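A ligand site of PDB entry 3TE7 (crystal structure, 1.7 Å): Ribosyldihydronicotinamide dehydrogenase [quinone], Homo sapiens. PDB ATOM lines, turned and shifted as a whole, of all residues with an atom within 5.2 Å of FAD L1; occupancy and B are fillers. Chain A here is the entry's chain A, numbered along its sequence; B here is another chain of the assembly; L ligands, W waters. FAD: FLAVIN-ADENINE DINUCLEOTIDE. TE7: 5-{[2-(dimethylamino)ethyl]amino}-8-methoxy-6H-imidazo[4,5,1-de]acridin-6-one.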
ATOM      1  N   HIS A  10      -0.850  30.123 -20.798  1.00  0.00           N
ATOM      2  CA  HIS A  10       0.591  30.142 -21.043  1.00  0.00           C
ATOM      3  C   HIS A  10       1.085  31.573 -21.069  1.00  0.00           C
ATOM      4  O   HIS A  10       0.408  32.471 -21.560  1.00  0.00           O
ATOM      5  CB  HIS A  10       0.959  29.422 -22.343  1.00  0.00           C
ATOM      6  CG  HIS A  10       2.390  28.979 -22.408  1.00  0.00           C
ATOM      7  ND1 HIS A  10       3.440  29.865 -22.554  1.00  0.00           N
ATOM      8  CD2 HIS A  10       2.949  27.754 -22.332  1.00  0.00           C
ATOM      9  CE1 HIS A  10       4.582  29.195 -22.577  1.00  0.00           C
ATOM     10  NE2 HIS A  10       4.307  27.907 -22.443  1.00  0.00           N
ATOM     11  N   LYS A  14       4.659  33.211 -28.165  1.00  0.00           N
ATOM     12  CA  LYS A  14       5.431  32.454 -29.155  1.00  0.00           C
ATOM     13  C   LYS A  14       5.644  30.990 -28.789  1.00  0.00           C
ATOM     14  O   LYS A  14       6.335  30.260 -29.501  1.00  0.00           O
ATOM     15  CB  LYS A  14       6.790  33.118 -29.365  1.00  0.00           C
ATOM     16  CG  LYS A  14       6.717  34.577 -29.752  1.00  0.00           C
ATOM     17  CD  LYS A  14       8.124  35.172 -29.841  1.00  0.00           C
ATOM     18  CE  LYS A  14       8.102  36.662 -30.156  1.00  0.00           C
ATOM     19  NZ  LYS A  14       7.494  36.914 -31.493  1.00  0.00           N
ATOM     20  N   SER A  15       5.066  30.564 -27.670  1.00  0.00           N
ATOM     21  CA  SER A  15       5.249  29.195 -27.181  1.00  0.00           C
ATOM     22  C   SER A  15       4.525  28.208 -28.078  1.00  0.00           C
ATOM     23  O   SER A  15       3.720  28.608 -28.925  1.00  0.00           O
ATOM     24  CB  SER A  15       4.692  29.088 -25.761  1.00  0.00           C
ATOM     25  OG  SER A  15       3.284  29.355 -25.731  1.00  0.00           O
ATOM     26  N   PHE A  16       4.812  26.927 -27.911  1.00  0.00           N
ATOM     27  CA  PHE A  16       4.052  25.867 -28.560  1.00  0.00           C
ATOM     28  C   PHE A  16       2.560  25.956 -28.180  1.00  0.00           C
ATOM     29  O   PHE A  16       1.687  25.771 -29.048  1.00  0.00           O
ATOM     30  CB  PHE A  16       4.638  24.505 -28.188  1.00  0.00           C
ATOM     31  CG  PHE A  16       4.164  23.373 -29.061  1.00  0.00           C
ATOM     32  CD1 PHE A  16       4.624  23.241 -30.363  1.00  0.00           C
ATOM     33  CD2 PHE A  16       3.295  22.431 -28.562  1.00  0.00           C
ATOM     34  CE1 PHE A  16       4.193  22.202 -31.159  1.00  0.00           C
ATOM     35  CE2 PHE A  16       2.853  21.381 -29.367  1.00  0.00           C
ATOM     36  CZ  PHE A  16       3.309  21.268 -30.662  1.00  0.00           C
ATOM     37  N   ASN A  17       2.261  26.240 -26.911  1.00  0.00           N
ATOM     38  CA  ASN A  17       0.865  26.423 -26.490  1.00  0.00           C
ATOM     39  C   ASN A  17       0.226  27.595 -27.223  1.00  0.00           C
ATOM     40  O   ASN A  17      -0.927  27.513 -27.649  1.00  0.00           O
ATOM     41  CB  ASN A  17       0.755  26.632 -24.975  1.00  0.00           C
ATOM     42  CG  ASN A  17       0.639  25.320 -24.226  1.00  0.00           C
ATOM     43  OD1 ASN A  17      -0.467  24.852 -23.947  1.00  0.00           O
ATOM     44  ND2 ASN A  17       1.784  24.723 -23.889  1.00  0.00           N
ATOM     45  N   SER A  19       0.988  28.694 -30.137  1.00  0.00           N
ATOM     46  CA  SER A  19       0.733  28.257 -31.518  1.00  0.00           C
ATOM     47  C   SER A  19      -0.499  27.345 -31.629  1.00  0.00           C
ATOM     48  O   SER A  19      -1.252  27.420 -32.599  1.00  0.00           O
ATOM     49  CB  SER A  19       1.941  27.538 -32.107  1.00  0.00           C
ATOM     50  OG  SER A  19       3.038  28.431 -32.240  1.00  0.00           O
ATOM     51  N   PRO A 101       0.007  23.885 -20.779  1.00  0.00           N
ATOM     52  CA  PRO A 101       1.076  22.923 -20.493  1.00  0.00           C
ATOM     53  C   PRO A 101       0.789  22.185 -19.190  1.00  0.00           C
ATOM     54  O   PRO A 101       0.277  22.773 -18.231  1.00  0.00           O
ATOM     55  CB  PRO A 101       2.304  23.830 -20.336  1.00  0.00           C
ATOM     56  CG  PRO A 101       1.715  25.130 -19.734  1.00  0.00           C
ATOM     57  CD  PRO A 101       0.329  25.263 -20.368  1.00  0.00           C
ATOM     58  N   LEU A 102       1.086  20.892 -19.152  1.00  0.00           N
ATOM     59  CA  LEU A 102       0.892  20.098 -17.948  1.00  0.00           C
ATOM     60  C   LEU A 102       1.851  20.593 -16.878  1.00  0.00           C
ATOM     61  O   LEU A 102       3.058  20.653 -17.108  1.00  0.00           O
ATOM     62  CB  LEU A 102       1.177  18.610 -18.224  1.00  0.00           C
ATOM     63  CG  LEU A 102       0.712  17.576 -17.202  1.00  0.00           C
ATOM     64  CD1 LEU A 102      -0.804  17.550 -17.126  1.00  0.00           C
ATOM     65  CD2 LEU A 102       1.229  16.191 -17.575  1.00  0.00           C
ATOM     66  N   TYR A 103       1.313  20.931 -15.712  1.00  0.00           N
ATOM     67  CA  TYR A 103       2.128  21.307 -14.567  1.00  0.00           C
ATOM     68  C   TYR A 103       1.812  20.326 -13.434  1.00  0.00           C
ATOM     69  O   TYR A 103       0.677  20.312 -12.949  1.00  0.00           O
ATOM     70  CB  TYR A 103       1.785  22.724 -14.065  1.00  0.00           C
ATOM     71  CG  TYR A 103       2.427  23.904 -14.770  1.00  0.00           C
ATOM     72  CD1 TYR A 103       3.066  23.781 -16.007  1.00  0.00           C
ATOM     73  CD2 TYR A 103       2.406  25.172 -14.179  1.00  0.00           C
ATOM     74  CE1 TYR A 103       3.646  24.893 -16.641  1.00  0.00           C
ATOM     75  CE2 TYR A 103       2.982  26.263 -14.782  1.00  0.00           C
ATOM     76  CZ  TYR A 103       3.595  26.131 -16.008  1.00  0.00           C
ATOM     77  OH  TYR A 103       4.164  27.244 -16.581  1.00  0.00           O
ATOM     78  N   TRP A 104       2.803  19.543 -13.019  1.00  0.00           N
ATOM     79  CA  TRP A 104       2.619  18.600 -11.917  1.00  0.00           C
ATOM     80  C   TRP A 104       1.387  17.734 -12.108  1.00  0.00           C
ATOM     81  O   TRP A 104       0.515  17.636 -11.224  1.00  0.00           O
ATOM     82  CB  TRP A 104       2.598  19.326 -10.563  1.00  0.00           C
ATOM     83  CG  TRP A 104       3.940  19.927 -10.263  1.00  0.00           C
ATOM     84  CD1 TRP A 104       4.233  21.245 -10.097  1.00  0.00           C
ATOM     85  CD2 TRP A 104       5.176  19.215 -10.114  1.00  0.00           C
ATOM     86  NE1 TRP A 104       5.584  21.403  -9.846  1.00  0.00           N
ATOM     87  CE2 TRP A 104       6.179  20.170  -9.855  1.00  0.00           C
ATOM     88  CE3 TRP A 104       5.535  17.859 -10.174  1.00  0.00           C
ATOM     89  CZ2 TRP A 104       7.515  19.817  -9.657  1.00  0.00           C
ATOM     90  CZ3 TRP A 104       6.855  17.514  -9.977  1.00  0.00           C
ATOM     91  CH2 TRP A 104       7.841  18.487  -9.719  1.00  0.00           C
ATOM     92  N   PHE A 105       1.361  17.068 -13.273  1.00  0.00           N
ATOM     93  CA  PHE A 105       0.305  16.120 -13.629  1.00  0.00           C
ATOM     94  C   PHE A 105      -1.084  16.772 -13.619  1.00  0.00           C
ATOM     95  O   PHE A 105      -2.084  16.071 -13.447  1.00  0.00           O
ATOM     96  CB  PHE A 105       0.297  14.912 -12.684  1.00  0.00           C
ATOM     97  CG  PHE A 105       1.244  13.798 -13.076  1.00  0.00           C
ATOM     98  CD1 PHE A 105       2.429  14.075 -13.722  1.00  0.00           C
ATOM     99  CD2 PHE A 105       0.924  12.477 -12.795  1.00  0.00           C
ATOM    100  CE1 PHE A 105       3.289  13.042 -14.092  1.00  0.00           C
ATOM    101  CE2 PHE A 105       1.789  11.443 -13.156  1.00  0.00           C
ATOM    102  CZ  PHE A 105       2.972  11.729 -13.798  1.00  0.00           C
ATOM    103  N   THR A 146      -0.040  19.974 -23.409  1.00  0.00           N
ATOM    104  CA  THR A 146       1.313  19.699 -23.875  1.00  0.00           C
ATOM    105  C   THR A 146       2.114  19.198 -22.666  1.00  0.00           C
ATOM    106  O   THR A 146       1.813  19.557 -21.537  1.00  0.00           O
ATOM    107  CB  THR A 146       1.999  20.966 -24.448  1.00  0.00           C
ATOM    108  OG1 THR A 146       2.172  21.932 -23.424  1.00  0.00           O
ATOM    109  CG2 THR A 146       1.175  21.573 -25.568  1.00  0.00           C
ATOM    110  N   THR A 147       3.139  18.388 -22.909  1.00  0.00           N
ATOM    111  CA  THR A 147       3.917  17.821 -21.815  1.00  0.00           C
ATOM    112  C   THR A 147       5.416  17.964 -22.005  1.00  0.00           C
ATOM    113  O   THR A 147       5.909  18.227 -23.107  1.00  0.00           O
ATOM    114  CB  THR A 147       3.628  16.308 -21.654  1.00  0.00           C
ATOM    115  OG1 THR A 147       4.123  15.614 -22.806  1.00  0.00           O
ATOM    116  CG2 THR A 147       2.128  16.056 -21.530  1.00  0.00           C
ATOM    117  N   GLY A 148       6.153  17.774 -20.917  1.00  0.00           N
ATOM    118  CA  GLY A 148       7.588  17.562 -21.004  1.00  0.00           C
ATOM    119  C   GLY A 148       7.922  16.112 -21.295  1.00  0.00           C
ATOM    120  O   GLY A 148       8.795  15.817 -22.114  1.00  0.00           O
ATOM    121  N   GLY A 149       7.237  15.198 -20.617  1.00  0.00           N
ATOM    122  CA  GLY A 149       7.469  13.777 -20.799  1.00  0.00           C
ATOM    123  C   GLY A 149       7.062  13.238 -22.166  1.00  0.00           C
ATOM    124  O   GLY A 149       6.143  13.752 -22.803  1.00  0.00           O
ATOM    125  N   TYR A 154       4.657   8.118 -20.644  1.00  0.00           N
ATOM    126  CA  TYR A 154       3.255   8.118 -20.224  1.00  0.00           C
ATOM    127  C   TYR A 154       2.477   6.890 -20.720  1.00  0.00           C
ATOM    128  O   TYR A 154       1.407   7.021 -21.298  1.00  0.00           O
ATOM    129  CB  TYR A 154       2.546   9.389 -20.703  1.00  0.00           C
ATOM    130  CG  TYR A 154       2.876  10.591 -19.849  1.00  0.00           C
ATOM    131  CD1 TYR A 154       2.364  10.719 -18.570  1.00  0.00           C
ATOM    132  CD2 TYR A 154       3.707  11.605 -20.328  1.00  0.00           C
ATOM    133  CE1 TYR A 154       2.656  11.817 -17.788  1.00  0.00           C
ATOM    134  CE2 TYR A 154       4.008  12.706 -19.549  1.00  0.00           C
ATOM    135  CZ  TYR A 154       3.474  12.812 -18.286  1.00  0.00           C
ATOM    136  OH  TYR A 154       3.764  13.896 -17.494  1.00  0.00           O
ATOM    137  N   ASN A 160       5.851   7.333 -15.589  1.00  0.00           N
ATOM    138  CA  ASN A 160       4.790   8.279 -15.290  1.00  0.00           C
ATOM    139  C   ASN A 160       3.395   7.651 -15.257  1.00  0.00           C
ATOM    140  O   ASN A 160       2.426   8.315 -14.912  1.00  0.00           O
ATOM    141  CB  ASN A 160       4.768   9.420 -16.313  1.00  0.00           C
ATOM    142  CG  ASN A 160       5.947  10.353 -16.173  1.00  0.00           C
ATOM    143  OD1 ASN A 160       6.640  10.338 -15.162  1.00  0.00           O
ATOM    144  ND2 ASN A 160       6.157  11.189 -17.185  1.00  0.00           N
ATOM    145  N   PRO A 191       7.004  18.550 -26.914  1.00  0.00           N
ATOM    146  CA  PRO A 191       7.411  19.426 -28.020  1.00  0.00           C
ATOM    147  C   PRO A 191       8.838  19.973 -27.871  1.00  0.00           C
ATOM    148  O   PRO A 191       9.499  20.222 -28.874  1.00  0.00           O
ATOM    149  CB  PRO A 191       6.380  20.552 -27.978  1.00  0.00           C
ATOM    150  CG  PRO A 191       5.803  20.512 -26.579  1.00  0.00           C
ATOM    151  CD  PRO A 191       5.794  19.047 -26.234  1.00  0.00           C
ATOM    152  N   GLU A 192       9.304  20.174 -26.646  1.00  0.00           N
ATOM    153  CA  GLU A 192      10.625  20.742 -26.432  1.00  0.00           C
ATOM    154  C   GLU A 192      11.744  19.863 -27.013  1.00  0.00           C
ATOM    155  O   GLU A 192      12.767  20.385 -27.456  1.00  0.00           O
ATOM    156  CB  GLU A 192      10.855  21.045 -24.944  1.00  0.00           C
ATOM    157  CG  GLU A 192      10.012  22.213 -24.442  1.00  0.00           C
ATOM    158  CD  GLU A 192      10.012  22.352 -22.937  1.00  0.00           C
ATOM    159  OE1 GLU A 192      10.679  23.272 -22.419  1.00  0.00           O
ATOM    160  OE2 GLU A 192       9.314  21.558 -22.273  1.00  0.00           O
ATOM    161  N   GLU A 196      11.857  19.864 -35.459  1.00  0.00           N
ATOM    162  CA  GLU A 196      11.094  20.948 -36.063  1.00  0.00           C
ATOM    163  C   GLU A 196       9.934  20.407 -36.882  1.00  0.00           C
ATOM    164  O   GLU A 196       8.816  20.935 -36.832  1.00  0.00           O
ATOM    165  CB  GLU A 196      12.000  21.812 -36.942  1.00  0.00           C
ATOM    166  CG  GLU A 196      11.302  22.977 -37.627  1.00  0.00           C
ATOM    167  CD  GLU A 196      10.913  24.080 -36.654  1.00  0.00           C
ATOM    168  OE1 GLU A 196      11.170  23.927 -35.438  1.00  0.00           O
ATOM    169  OE2 GLU A 196      10.364  25.102 -37.112  1.00  0.00           O
ATOM    170  N   ARG A 199       7.327  18.949 -34.446  1.00  0.00           N
ATOM    171  CA  ARG A 199       6.531  20.037 -33.893  1.00  0.00           C
ATOM    172  C   ARG A 199       5.483  20.498 -34.907  1.00  0.00           C
ATOM    173  O   ARG A 199       4.293  20.587 -34.588  1.00  0.00           O
ATOM    174  CB  ARG A 199       7.399  21.234 -33.512  1.00  0.00           C
ATOM    175  CG  ARG A 199       8.352  21.003 -32.340  1.00  0.00           C
ATOM    176  CD  ARG A 199       9.176  22.257 -32.107  1.00  0.00           C
ATOM    177  NE  ARG A 199      10.415  21.975 -31.402  1.00  0.00           N
ATOM    178  CZ  ARG A 199      11.564  22.616 -31.621  1.00  0.00           C
ATOM    179  NH1 ARG A 199      11.615  23.569 -32.536  1.00  0.00           N
ATOM    180  NH2 ARG A 199      12.652  22.294 -30.933  1.00  0.00           N
ATOM    181  N   LYS A 200       5.921  20.778 -36.137  1.00  0.00           N
ATOM    182  CA  LYS A 200       4.981  21.243 -37.155  1.00  0.00           C
ATOM    183  C   LYS A 200       3.883  20.218 -37.429  1.00  0.00           C
ATOM    184  O   LYS A 200       2.741  20.590 -37.724  1.00  0.00           O
ATOM    185  CB  LYS A 200       5.713  21.617 -38.445  1.00  0.00           C
ATOM    186  CG  LYS A 200       6.477  22.922 -38.352  1.00  0.00           C
ATOM    187  CD  LYS A 200       7.314  23.175 -39.592  1.00  0.00           C
ATOM    188  CE  LYS A 200       8.252  24.357 -39.392  1.00  0.00           C
ATOM    189  NZ  LYS A 200       9.229  24.466 -40.513  1.00  0.00           N
ATOM    190  N   VAL A 203       1.193  20.474 -34.607  1.00  0.00           N
ATOM    191  CA  VAL A 203       0.340  21.646 -34.761  1.00  0.00           C
ATOM    192  C   VAL A 203      -0.669  21.410 -35.878  1.00  0.00           C
ATOM    193  O   VAL A 203      -1.851  21.743 -35.759  1.00  0.00           O
ATOM    194  CB  VAL A 203       1.163  22.923 -35.059  1.00  0.00           C
ATOM    195  CG1 VAL A 203       0.250  24.090 -35.343  1.00  0.00           C
ATOM    196  CG2 VAL A 203       2.083  23.236 -33.874  1.00  0.00           C
ATOM    197  N   ASN B  65      10.444  31.367 -21.104  1.00  0.00           N
ATOM    198  CA  ASN B  65      10.236  29.961 -20.813  1.00  0.00           C
ATOM    199  C   ASN B  65      10.350  29.795 -19.310  1.00  0.00           C
ATOM    200  O   ASN B  65      11.452  29.895 -18.766  1.00  0.00           O
ATOM    201  CB  ASN B  65      11.312  29.139 -21.541  1.00  0.00           C
ATOM    202  CG  ASN B  65      11.131  27.646 -21.403  1.00  0.00           C
ATOM    203  OD1 ASN B  65      10.940  27.119 -20.303  1.00  0.00           O
ATOM    204  ND2 ASN B  65      11.176  26.951 -22.527  1.00  0.00           N
ATOM    205  N   TYR B  66       9.222  29.585 -18.632  1.00  0.00           N
ATOM    206  CA  TYR B  66       9.214  29.575 -17.164  1.00  0.00           C
ATOM    207  C   TYR B  66      10.172  28.528 -16.575  1.00  0.00           C
ATOM    208  O   TYR B  66      10.936  28.823 -15.658  1.00  0.00           O
ATOM    209  CB  TYR B  66       7.786  29.370 -16.617  1.00  0.00           C
ATOM    210  CG  TYR B  66       7.721  29.561 -15.116  1.00  0.00           C
ATOM    211  CD1 TYR B  66       7.680  30.838 -14.569  1.00  0.00           C
ATOM    212  CD2 TYR B  66       7.724  28.472 -14.241  1.00  0.00           C
ATOM    213  CE1 TYR B  66       7.641  31.026 -13.181  1.00  0.00           C
ATOM    214  CE2 TYR B  66       7.693  28.646 -12.871  1.00  0.00           C
ATOM    215  CZ  TYR B  66       7.653  29.931 -12.346  1.00  0.00           C
ATOM    216  OH  TYR B  66       7.631  30.108 -10.979  1.00  0.00           O
ATOM    217  N   GLY B  67      10.113  27.306 -17.098  1.00  0.00           N
ATOM    218  CA  GLY B  67      10.963  26.241 -16.597  1.00  0.00           C
ATOM    219  C   GLY B  67      12.445  26.550 -16.745  1.00  0.00           C
ATOM    220  O   GLY B  67      13.241  26.368 -15.816  1.00  0.00           O
ATOM    221  N   ASP B 116       3.827  24.675  -8.005  1.00  0.00           N
ATOM    222  CA  ASP B 116       4.344  25.101  -9.309  1.00  0.00           C
ATOM    223  C   ASP B 116       5.604  25.966  -9.165  1.00  0.00           C
ATOM    224  O   ASP B 116       6.575  25.829  -9.941  1.00  0.00           O
ATOM    225  CB  ASP B 116       3.301  25.952 -10.056  1.00  0.00           C
ATOM    226  CG  ASP B 116       2.074  25.175 -10.500  1.00  0.00           C
ATOM    227  OD1 ASP B 116       2.050  23.906 -10.456  1.00  0.00           O
ATOM    228  OD2 ASP B 116       1.118  25.867 -10.905  1.00  0.00           O
ATOM    229  N   GLY B 173       2.939  11.988  -9.131  1.00  0.00           N
ATOM    230  CA  GLY B 173       3.367  12.980 -10.111  1.00  0.00           C
ATOM    231  C   GLY B 173       4.141  14.128  -9.495  1.00  0.00           C
ATOM    232  O   GLY B 173       4.960  14.750 -10.171  1.00  0.00           O
HETATM  233  PA  FAD L   1       7.731  25.580 -25.822  1.00  0.00           P
HETATM  234  O1A FAD L   1       7.149  26.949 -26.004  1.00  0.00           O
HETATM  235  O2A FAD L   1       9.061  25.636 -25.078  1.00  0.00           O
HETATM  236  O5B FAD L   1       7.887  24.946 -27.242  1.00  0.00           O
HETATM  237  C5B FAD L   1       8.998  24.141 -27.580  1.00  0.00           C
HETATM  238  C4B FAD L   1       9.453  24.565 -28.957  1.00  0.00           C
HETATM  239  O4B FAD L   1       8.383  24.564 -29.909  1.00  0.00           O
HETATM  240  C3B FAD L   1      10.020  25.958 -28.946  1.00  0.00           C
HETATM  241  O3B FAD L   1      11.281  25.978 -29.533  1.00  0.00           O
HETATM  242  C2B FAD L   1       9.122  26.775 -29.755  1.00  0.00           C
HETATM  243  O2B FAD L   1       9.798  27.749 -30.461  1.00  0.00           O
HETATM  244  C1B FAD L   1       8.569  25.716 -30.678  1.00  0.00           C
HETATM  245  N9A FAD L   1       7.420  26.150 -31.427  1.00  0.00           N
HETATM  246  C8A FAD L   1       6.420  27.137 -31.080  1.00  0.00           C
HETATM  247  N7A FAD L   1       5.493  27.215 -32.116  1.00  0.00           N
HETATM  248  C5A FAD L   1       5.888  26.312 -33.074  1.00  0.00           C
HETATM  249  C6A FAD L   1       5.307  26.057 -34.235  1.00  0.00           C
HETATM  250  N6A FAD L   1       4.063  26.627 -34.588  1.00  0.00           N
HETATM  251  N1A FAD L   1       5.884  25.085 -35.045  1.00  0.00           N
HETATM  252  C2A FAD L   1       7.190  24.643 -34.682  1.00  0.00           C
HETATM  253  N3A FAD L   1       7.622  24.803 -33.349  1.00  0.00           N
HETATM  254  C4A FAD L   1       7.014  25.689 -32.666  1.00  0.00           C
HETATM  255  N1  FAD L   1       5.769  17.992 -17.876  1.00  0.00           N
HETATM  256  C2  FAD L   1       5.225  16.662 -17.660  1.00  0.00           C
HETATM  257  O2  FAD L   1       5.308  15.752 -18.644  1.00  0.00           O
HETATM  258  N3  FAD L   1       4.622  16.336 -16.431  1.00  0.00           N
HETATM  259  C4  FAD L   1       4.546  17.276 -15.433  1.00  0.00           C
HETATM  260  O4  FAD L   1       3.964  16.977 -14.241  1.00  0.00           O
HETATM  261  C4X FAD L   1       5.095  18.628 -15.646  1.00  0.00           C
HETATM  262  N5  FAD L   1       5.046  19.577 -14.659  1.00  0.00           N
HETATM  263  C5X FAD L   1       5.573  20.866 -14.897  1.00  0.00           C
HETATM  264  C6  FAD L   1       5.519  21.834 -13.903  1.00  0.00           C
HETATM  265  C7  FAD L   1       6.018  23.101 -14.088  1.00  0.00           C
HETATM  266  C7M FAD L   1       5.916  24.117 -12.973  1.00  0.00           C
HETATM  267  C8  FAD L   1       6.608  23.426 -15.323  1.00  0.00           C
HETATM  268  C8M FAD L   1       7.187  24.790 -15.592  1.00  0.00           C
HETATM  269  C9  FAD L   1       6.681  22.472 -16.311  1.00  0.00           C
HETATM  270  C9A FAD L   1       6.171  21.177 -16.149  1.00  0.00           C
HETATM  271  N10 FAD L   1       6.232  20.188 -17.173  1.00  0.00           N
HETATM  272  C10 FAD L   1       5.696  18.929 -16.902  1.00  0.00           C
HETATM  273  C1' FAD L   1       6.820  20.427 -18.514  1.00  0.00           C
HETATM  274  C2' FAD L   1       5.771  21.189 -19.354  1.00  0.00           C
HETATM  275  O2' FAD L   1       4.597  20.511 -19.489  1.00  0.00           O
HETATM  276  C3' FAD L   1       6.361  21.499 -20.715  1.00  0.00           C
HETATM  277  O3' FAD L   1       7.469  22.288 -20.538  1.00  0.00           O
HETATM  278  C4' FAD L   1       5.387  22.237 -21.673  1.00  0.00           C
HETATM  279  O4' FAD L   1       4.270  21.394 -21.924  1.00  0.00           O
HETATM  280  C5' FAD L   1       6.032  22.634 -22.963  1.00  0.00           C
HETATM  281  O5' FAD L   1       5.108  23.420 -23.722  1.00  0.00           O
HETATM  282  P   FAD L   1       5.488  24.870 -24.140  1.00  0.00           P
HETATM  283  O1P FAD L   1       4.366  25.490 -24.886  1.00  0.00           O
HETATM  284  O2P FAD L   1       5.900  25.663 -22.971  1.00  0.00           O
HETATM  285  O3P FAD L   1       6.734  24.549 -25.091  1.00  0.00           O
HETATM  286  CAA TE7 L   2       5.892  14.344 -13.704  1.00  0.00           C
HETATM  287  CAB TE7 L   2      13.199  22.207 -20.671  1.00  0.00           C
HETATM  288  CAC TE7 L   2      13.353  20.022 -21.632  1.00  0.00           C
HETATM  289  OAD TE7 L   2       9.383  17.615 -17.487  1.00  0.00           O
HETATM  290  CAE TE7 L   2       7.117  16.508 -13.324  1.00  0.00           C
HETATM  291  CAF TE7 L   2      10.626  21.658 -17.126  1.00  0.00           C
HETATM  292  CAG TE7 L   2      10.305  22.299 -15.920  1.00  0.00           C
HETATM  293  CAH TE7 L   2       7.523  17.834 -13.208  1.00  0.00           C
HETATM  294  CAI TE7 L   2       8.541  20.738 -13.232  1.00  0.00           C
HETATM  295  CAJ TE7 L   2       8.070  16.390 -15.543  1.00  0.00           C
HETATM  296  CAK TE7 L   2      11.304  20.321 -19.611  1.00  0.00           C
HETATM  297  CAL TE7 L   2      12.799  20.249 -19.306  1.00  0.00           C
HETATM  298  NAM TE7 L   2       9.138  21.848 -13.706  1.00  0.00           N
HETATM  299  NAN TE7 L   2      10.567  19.700 -18.492  1.00  0.00           N
HETATM  300  OAO TE7 L   2       6.989  14.504 -14.590  1.00  0.00           O
HETATM  301  CAP TE7 L   2       7.375  15.799 -14.493  1.00  0.00           C
HETATM  302  CAQ TE7 L   2      10.271  20.315 -17.359  1.00  0.00           C
HETATM  303  CAR TE7 L   2       9.164  18.295 -16.476  1.00  0.00           C
HETATM  304  CAS TE7 L   2       9.610  21.600 -14.936  1.00  0.00           C
HETATM  305  CAT TE7 L   2       8.479  17.714 -15.418  1.00  0.00           C
HETATM  306  CAU TE7 L   2       8.207  18.431 -14.251  1.00  0.00           C
HETATM  307  CAV TE7 L   2       9.574  19.625 -16.372  1.00  0.00           C
HETATM  308  CAW TE7 L   2       9.283  20.296 -15.207  1.00  0.00           C
HETATM  309  NAX TE7 L   2      13.595  20.814 -20.408  1.00  0.00           N
HETATM  310  NAY TE7 L   2       8.617  19.762 -14.148  1.00  0.00           N
HETATM  311  O   HOH W   1      11.563  25.725 -25.516  1.00  0.00           O
HETATM  312  O   HOH W   2       7.902  23.333 -10.677  1.00  0.00           O
HETATM  313  O   HOH W   3       2.966  26.003 -37.478  1.00  0.00           O
HETATM  314  O   HOH W   4       9.013  23.867 -18.813  1.00  0.00           O
HETATM  315  O   HOH W   5       8.814  29.110 -26.174  1.00  0.00           O
HETATM  316  O   HOH W   6       5.674  25.524 -20.153  1.00  0.00           O
HETATM  317  O   HOH W   7       8.977  29.842 -28.808  1.00  0.00           O
HETATM  318  O   HOH W   8       8.166  27.139 -22.314  1.00  0.00           O
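N1 of FAD L1 is in hydrogen-bond range of N of Gly 148 (3.1 Å).
The backbone NH (N) of Phe 16 lies within hydrogen-bond range of an oxygen (O1A) of FAD L1, at 3.0 Å.
An oxygen (O2) of FAD L1 sits at hydrogen-bond distance from the side-chain hydroxyl (OH) of Tyr 154, at 2.7 Å.
O2P of FAD L1 lies within hydrogen-bond range of NE2 of His 10.
O1P of FAD L1 is in hydrogen-bond range of ND2 of Asn 17, at 2.9 Å.
O3' of FAD L1 is in hydrogen-bond range of OE2 of Glu 192 (2.6 Å).
An oxygen (O2') of FAD L1 sits at hydrogen-bond distance from the backbone carbonyl oxygen (O) of Leu 102.
OG of Ser 19 is in hydrogen-bond range of N7A of FAD L1.
The backbone NH (N) of Trp 104 lies within hydrogen-bond range of a nitrogen (N5) of FAD L1 (2.8 Å).
An oxygen (O1P) of FAD L1 is in hydrogen-bond range of the backbone NH (N) of Asn 17, at 3.0 Å.
The backbone NH (N) of Gly 149 is in hydrogen-bond range of an oxygen (O2) of FAD L1 (2.8 Å).
An oxygen (O4') of FAD L1 sits at hydrogen-bond distance from the backbone NH (N) of Thr 147 (3.4 Å).
OG1 of Thr 146 sits at hydrogen-bond distance from O4' of FAD L1.
N of Phe 105 lies within hydrogen-bond range of O4 of FAD L1, 2.8 Å away.
The backbone carbonyl oxygen (O) of Thr 146 is in hydrogen-bond range of an oxygen (O4') of FAD L1, 3.1 Å away.
ND1 of His 10 sits at hydrogen-bond distance from OG of Ser 15 (3.2 Å).
The side-chain hydroxyl (OG) of Ser 19 is in hydrogen-bond range of the backbone carbonyl oxygen (O) of Ser 15 (3.4 Å).
The side-chain carboxylate (OE1) of Glu 196 lies within salt-bridge range of the guanidinium group (NH1) of Arg 199 (3.0 Å).
The backbone NH (N) of Gly 67 of chain B is in hydrogen-bond range of the side-chain amide oxygen (OD1) of Asn 65 of chain B (3.3 Å).
O of Gly 149 is in hydrogen-bond range of OG1 of Thr 147, at 2.7 Å.
NZ of Lys 200 lies within salt-bridge range of OE2 of Glu 196, at 3.6 Å.
The backbone carbonyl oxygen (O) of Thr 146 lies within hydrogen-bond range of the backbone NH (N) of Leu 102, at 2.8 Å.
The backbone carbonyl oxygen of Pro 191 is in hydrogen-bond range of the guanidinium group of Arg 199, 3.2 Å away.
Lys 14 touches FAD L1.
Ser 15 touches FAD L1 (CA to O1A, 3.2 Å).
CB of Pro 101 touches O4' of FAD L1, 3.5 Å away.
Tyr 103 touches FAD L1.
Arg 199 touches FAD L1.
CG of Lys 200 touches N1A of FAD L1, at 3.996 Å.
CG2 of Val 203 touches N6A of FAD L1, 3.99 Å away.
Asn 65 of chain B touches FAD L1 (ND2 to O2A, 3.6 Å).
CD2 of Tyr 66 of chain B touches C8M of FAD L1, at 3.96 Å.
Asp 116 of chain B touches FAD L1 (O to C7M, 3.5 Å).
Hydrophobic or aromatic side chains within 4 Å of FAD L1: His 10, Phe 16, Pro 101, Leu 102, Tyr 103, Phe 105, Tyr 154, Val 203 and Tyr 66 of chain B.
Water W1 lies within hydrogen-bond range of O2A of FAD L1 (2.5 Å) and ND2 of Asn 65 of chain B (3.3 Å).
Water W8 bridges an oxygen (O2P) of FAD L1 (2.8 Å) and the side-chain amide nitrogen (ND2) of Asn 65 of chain B (3.0 Å).
Water W7 lies within hydrogen-bond range of O of Lys 14 (2.8 Å) and O2B of FAD L1 (2.8 Å).
Water W2 bridges the backbone carbonyl oxygen of Asp 116 of chain B and the indole nitrogen of Trp 104.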
